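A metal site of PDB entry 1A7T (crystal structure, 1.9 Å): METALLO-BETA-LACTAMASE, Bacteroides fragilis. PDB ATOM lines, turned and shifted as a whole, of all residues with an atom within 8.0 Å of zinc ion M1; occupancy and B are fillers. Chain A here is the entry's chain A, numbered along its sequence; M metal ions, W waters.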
ATOM      1  N   VAL A  35      -4.549   9.748  29.055  1.00  0.00           N
ATOM      2  CA  VAL A  35      -5.057   9.416  27.703  1.00  0.00           C
ATOM      3  C   VAL A  35      -4.637   8.034  27.282  1.00  0.00           C
ATOM      4  O   VAL A  35      -3.449   7.746  27.386  1.00  0.00           O
ATOM      5  CB  VAL A  35      -4.381  10.458  26.767  1.00  0.00           C
ATOM      6  CG1 VAL A  35      -4.584  10.185  25.297  1.00  0.00           C
ATOM      7  CG2 VAL A  35      -4.956  11.817  27.118  1.00  0.00           C
ATOM      8  N   PRO A  36      -5.572   7.202  26.831  1.00  0.00           N
ATOM      9  CA  PRO A  36      -5.294   5.867  26.321  1.00  0.00           C
ATOM     10  C   PRO A  36      -5.000   6.025  24.810  1.00  0.00           C
ATOM     11  O   PRO A  36      -5.871   6.631  24.143  1.00  0.00           O
ATOM     12  CB  PRO A  36      -6.644   5.130  26.456  1.00  0.00           C
ATOM     13  CG  PRO A  36      -7.676   6.176  26.628  1.00  0.00           C
ATOM     14  CD  PRO A  36      -7.027   7.518  26.747  1.00  0.00           C
ATOM     15  N   SER A  37      -3.876   5.546  24.342  1.00  0.00           N
ATOM     16  CA  SER A  37      -3.509   5.644  22.906  1.00  0.00           C
ATOM     17  C   SER A  37      -3.430   4.181  22.406  1.00  0.00           C
ATOM     18  O   SER A  37      -2.910   3.361  23.162  1.00  0.00           O
ATOM     19  CB  SER A  37      -2.196   6.325  22.745  1.00  0.00           C
ATOM     20  OG  SER A  37      -2.451   7.696  23.108  1.00  0.00           O
ATOM     21  N   ASN A  38      -4.000   3.918  21.238  1.00  0.00           N
ATOM     22  CA  ASN A  38      -4.068   2.554  20.737  1.00  0.00           C
ATOM     23  C   ASN A  38      -3.147   2.319  19.555  1.00  0.00           C
ATOM     24  O   ASN A  38      -2.909   3.228  18.788  1.00  0.00           O
ATOM     25  CB  ASN A  38      -5.490   2.334  20.101  1.00  0.00           C
ATOM     26  CG  ASN A  38      -6.597   2.236  21.074  1.00  0.00           C
ATOM     27  OD1 ASN A  38      -6.358   1.801  22.196  1.00  0.00           O
ATOM     28  ND2 ASN A  38      -7.856   2.556  20.754  1.00  0.00           N
ATOM     29  N   ASP A  52       1.642   2.255  14.956  1.00  0.00           N
ATOM     30  CA  ASP A  52       1.741   3.295  15.918  1.00  0.00           C
ATOM     31  C   ASP A  52       2.582   2.831  17.111  1.00  0.00           C
ATOM     32  O   ASP A  52       2.633   1.663  17.534  1.00  0.00           O
ATOM     33  CB  ASP A  52       0.411   3.786  16.549  1.00  0.00           C
ATOM     34  CG  ASP A  52      -0.393   4.701  15.647  1.00  0.00           C
ATOM     35  OD1 ASP A  52      -0.033   4.948  14.481  1.00  0.00           O
ATOM     36  OD2 ASP A  52      -1.422   5.264  16.050  1.00  0.00           O
ATOM     37  N   ASN A  81       0.182   6.149  12.087  1.00  0.00           N
ATOM     38  CA  ASN A  81      -1.029   6.689  11.503  1.00  0.00           C
ATOM     39  C   ASN A  81      -0.892   8.129  11.026  1.00  0.00           C
ATOM     40  O   ASN A  81      -1.496   8.486  10.050  1.00  0.00           O
ATOM     41  CB  ASN A  81      -2.123   6.672  12.545  1.00  0.00           C
ATOM     42  CG  ASN A  81      -3.444   6.997  11.936  1.00  0.00           C
ATOM     43  OD1 ASN A  81      -3.975   8.082  12.131  1.00  0.00           O
ATOM     44  ND2 ASN A  81      -3.980   6.062  11.120  1.00  0.00           N
ATOM     45  N   HIS A  82      -0.157   8.995  11.730  1.00  0.00           N
ATOM     46  CA  HIS A  82       0.024  10.380  11.356  1.00  0.00           C
ATOM     47  C   HIS A  82       1.203  10.930  12.191  1.00  0.00           C
ATOM     48  O   HIS A  82       1.859  10.094  12.858  1.00  0.00           O
ATOM     49  CB  HIS A  82      -1.198  11.283  11.491  1.00  0.00           C
ATOM     50  CG  HIS A  82      -1.878  11.296  12.834  1.00  0.00           C
ATOM     51  ND1 HIS A  82      -2.606  10.221  13.338  1.00  0.00           N
ATOM     52  CD2 HIS A  82      -1.949  12.257  13.752  1.00  0.00           C
ATOM     53  CE1 HIS A  82      -3.095  10.536  14.534  1.00  0.00           C
ATOM     54  NE2 HIS A  82      -2.673  11.765  14.807  1.00  0.00           N
ATOM     55  N   HIS A  84       1.501  12.804  14.995  1.00  0.00           N
ATOM     56  CA  HIS A  84       1.414  13.123  16.425  1.00  0.00           C
ATOM     57  C   HIS A  84       2.127  12.126  17.308  1.00  0.00           C
ATOM     58  O   HIS A  84       2.521  11.023  16.899  1.00  0.00           O
ATOM     59  CB  HIS A  84      -0.007  13.330  16.891  1.00  0.00           C
ATOM     60  CG  HIS A  84      -0.784  14.488  16.392  1.00  0.00           C
ATOM     61  ND1 HIS A  84      -2.147  14.516  16.368  1.00  0.00           N
ATOM     62  CD2 HIS A  84      -0.417  15.665  15.850  1.00  0.00           C
ATOM     63  CE1 HIS A  84      -2.632  15.673  15.884  1.00  0.00           C
ATOM     64  NE2 HIS A  84      -1.574  16.393  15.590  1.00  0.00           N
ATOM     65  N   GLY A  85       2.357  12.570  18.590  1.00  0.00           N
ATOM     66  CA  GLY A  85       3.112  11.780  19.529  1.00  0.00           C
ATOM     67  C   GLY A  85       2.512  10.440  19.845  1.00  0.00           C
ATOM     68  O   GLY A  85       3.266   9.513  20.164  1.00  0.00           O
ATOM     69  N   ASP A  86       1.184  10.341  19.814  1.00  0.00           N
ATOM     70  CA  ASP A  86       0.602   9.030  20.083  1.00  0.00           C
ATOM     71  C   ASP A  86       0.716   8.090  18.881  1.00  0.00           C
ATOM     72  O   ASP A  86       0.084   7.042  18.890  1.00  0.00           O
ATOM     73  CB  ASP A  86      -0.839   9.167  20.513  1.00  0.00           C
ATOM     74  CG  ASP A  86      -1.697  10.053  19.636  1.00  0.00           C
ATOM     75  OD1 ASP A  86      -1.328  11.170  19.227  1.00  0.00           O
ATOM     76  OD2 ASP A  86      -2.831   9.542  19.284  1.00  0.00           O
ATOM     77  N   CYS A  87       1.439   8.413  17.833  1.00  0.00           N
ATOM     78  CA  CYS A  87       1.722   7.621  16.688  1.00  0.00           C
ATOM     79  C   CYS A  87       3.209   7.356  16.484  1.00  0.00           C
ATOM     80  O   CYS A  87       3.595   6.273  16.136  1.00  0.00           O
ATOM     81  CB  CYS A  87       1.201   8.250  15.370  1.00  0.00           C
ATOM     82  SG  CYS A  87      -0.558   8.694  15.510  1.00  0.00           S
ATOM     83  N   HIS A 145      -8.769  13.923  11.154  1.00  0.00           N
ATOM     84  CA  HIS A 145      -8.252  14.353  12.448  1.00  0.00           C
ATOM     85  C   HIS A 145      -6.930  15.083  12.300  1.00  0.00           C
ATOM     86  O   HIS A 145      -6.586  16.057  12.993  1.00  0.00           O
ATOM     87  CB  HIS A 145      -8.074  13.139  13.386  1.00  0.00           C
ATOM     88  CG  HIS A 145      -7.028  13.389  14.414  1.00  0.00           C
ATOM     89  ND1 HIS A 145      -7.324  13.997  15.617  1.00  0.00           N
ATOM     90  CD2 HIS A 145      -5.716  13.081  14.476  1.00  0.00           C
ATOM     91  CE1 HIS A 145      -6.228  14.098  16.391  1.00  0.00           C
ATOM     92  NE2 HIS A 145      -5.249  13.562  15.722  1.00  0.00           N
ATOM     93  N   GLY A 163      -7.261   4.487  13.219  1.00  0.00           N
ATOM     94  CA  GLY A 163      -6.484   5.585  13.811  1.00  0.00           C
ATOM     95  C   GLY A 163      -7.360   6.688  14.327  1.00  0.00           C
ATOM     96  O   GLY A 163      -8.596   6.612  14.418  1.00  0.00           O
ATOM     97  N   CYS A 164      -6.738   7.858  14.634  1.00  0.00           N
ATOM     98  CA  CYS A 164      -7.446   8.977  15.164  1.00  0.00           C
ATOM     99  C   CYS A 164      -8.519   9.642  14.344  1.00  0.00           C
ATOM    100  O   CYS A 164      -9.314  10.369  14.973  1.00  0.00           O
ATOM    101  CB  CYS A 164      -6.429  10.025  15.683  1.00  0.00           C
ATOM    102  SG  CYS A 164      -5.381   9.134  16.898  1.00  0.00           S
ATOM    103  N   MET A 165      -8.595   9.404  13.046  1.00  0.00           N
ATOM    104  CA  MET A 165      -9.693   9.983  12.263  1.00  0.00           C
ATOM    105  C   MET A 165     -11.022   9.348  12.707  1.00  0.00           C
ATOM    106  O   MET A 165     -12.106   9.883  12.451  1.00  0.00           O
ATOM    107  CB  MET A 165      -9.481   9.747  10.754  1.00  0.00           C
ATOM    108  CG  MET A 165     -10.004   8.392  10.312  1.00  0.00           C
ATOM    109  SD  MET A 165     -10.121   8.249   8.521  1.00  0.00           S
ATOM    110  CE  MET A 165      -8.371   8.267   8.059  1.00  0.00           C
ATOM    111  N   LEU A 166     -10.977   8.280  13.500  1.00  0.00           N
ATOM    112  CA  LEU A 166     -12.165   7.667  14.045  1.00  0.00           C
ATOM    113  C   LEU A 166     -12.248   7.835  15.560  1.00  0.00           C
ATOM    114  O   LEU A 166     -11.226   7.654  16.289  1.00  0.00           O
ATOM    115  CB  LEU A 166     -12.204   6.147  13.788  1.00  0.00           C
ATOM    116  CG  LEU A 166     -12.276   5.669  12.327  1.00  0.00           C
ATOM    117  CD1 LEU A 166     -12.626   4.162  12.326  1.00  0.00           C
ATOM    118  CD2 LEU A 166     -13.383   6.328  11.530  1.00  0.00           C
ATOM    119  N   LYS A 167     -13.421   8.132  16.075  1.00  0.00           N
ATOM    120  CA  LYS A 167     -13.713   8.247  17.483  1.00  0.00           C
ATOM    121  C   LYS A 167     -14.432   6.970  17.954  1.00  0.00           C
ATOM    122  O   LYS A 167     -15.187   6.272  17.220  1.00  0.00           O
ATOM    123  CB  LYS A 167     -14.563   9.462  17.794  1.00  0.00           C
ATOM    124  CG  LYS A 167     -14.092  10.851  17.330  1.00  0.00           C
ATOM    125  CD  LYS A 167     -12.760  11.158  17.910  1.00  0.00           C
ATOM    126  CE  LYS A 167     -12.187  12.534  17.467  1.00  0.00           C
ATOM    127  NZ  LYS A 167     -11.103  12.822  18.468  1.00  0.00           N
ATOM    128  N   ASN A 176      -9.300  17.220  19.802  1.00  0.00           N
ATOM    129  CA  ASN A 176      -8.208  18.050  19.327  1.00  0.00           C
ATOM    130  C   ASN A 176      -8.219  18.257  17.819  1.00  0.00           C
ATOM    131  O   ASN A 176      -7.987  17.277  17.062  1.00  0.00           O
ATOM    132  CB  ASN A 176      -6.900  17.273  19.727  1.00  0.00           C
ATOM    133  CG  ASN A 176      -5.718  18.116  19.228  1.00  0.00           C
ATOM    134  OD1 ASN A 176      -5.857  19.346  19.126  1.00  0.00           O
ATOM    135  ND2 ASN A 176      -4.661  17.378  18.895  1.00  0.00           N
ATOM    136  N   PRO A 204     -10.015   2.472  16.628  1.00  0.00           N
ATOM    137  CA  PRO A 204      -9.765   3.918  16.550  1.00  0.00           C
ATOM    138  C   PRO A 204      -8.439   4.231  17.240  1.00  0.00           C
ATOM    139  O   PRO A 204      -7.830   3.364  17.834  1.00  0.00           O
ATOM    140  CB  PRO A 204     -10.983   4.440  17.353  1.00  0.00           C
ATOM    141  CG  PRO A 204     -11.088   3.414  18.464  1.00  0.00           C
ATOM    142  CD  PRO A 204     -10.749   2.079  17.813  1.00  0.00           C
ATOM    143  N   GLY A 205      -8.020   5.509  17.234  1.00  0.00           N
ATOM    144  CA  GLY A 205      -6.817   6.012  17.808  1.00  0.00           C
ATOM    145  C   GLY A 205      -6.872   6.006  19.333  1.00  0.00           C
ATOM    146  O   GLY A 205      -5.837   5.813  19.932  1.00  0.00           O
ATOM    147  N   HIS A 206      -8.047   6.194  19.902  1.00  0.00           N
ATOM    148  CA  HIS A 206      -8.227   6.208  21.348  1.00  0.00           C
ATOM    149  C   HIS A 206      -9.579   5.582  21.736  1.00  0.00           C
ATOM    150  O   HIS A 206     -10.594   5.835  21.056  1.00  0.00           O
ATOM    151  CB  HIS A 206      -8.239   7.653  21.894  1.00  0.00           C
ATOM    152  CG  HIS A 206      -7.066   8.466  21.464  1.00  0.00           C
ATOM    153  ND1 HIS A 206      -5.846   8.468  22.127  1.00  0.00           N
ATOM    154  CD2 HIS A 206      -6.907   9.276  20.356  1.00  0.00           C
ATOM    155  CE1 HIS A 206      -4.982   9.216  21.472  1.00  0.00           C
ATOM    156  NE2 HIS A 206      -5.590   9.711  20.403  1.00  0.00           N
HETATM  157 ZN    ZN M   1      -4.734  10.499  18.518  1.00  0.00          ZN
HETATM  158 ZN    ZN M   2      -3.413  12.924  16.388  1.00  0.00          ZN
HETATM  159  O   HOH W   1      -6.609  11.852  18.520  1.00  0.00           O
HETATM  160  O   HOH W   2      -3.566  12.273  18.205  1.00  0.00           O
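A ring nitrogen (ND1) of His 206 lies within hydrogen-bond range of the backbone carbonyl oxygen of Pro 36.
Three residues have an atom within 4 Å of zinc ion M1: Asp 86, Cys 164 and His 206.
Zinc ion M1 is bound by water W2 (2.1 Å).
Zinc ion M1 is bound by SG of Cys 164 (2.2 Å).
Zinc ion M1 is bound by NE2 of His 206, at 2.2 Å.
Zinc ion M1 is bound by OD2 of Asp 86 (2.3 Å).
Water W1 is bound to zinc ion M1 (2.3 Å).
Zinc ion M1 has five donor atoms within binding distance.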
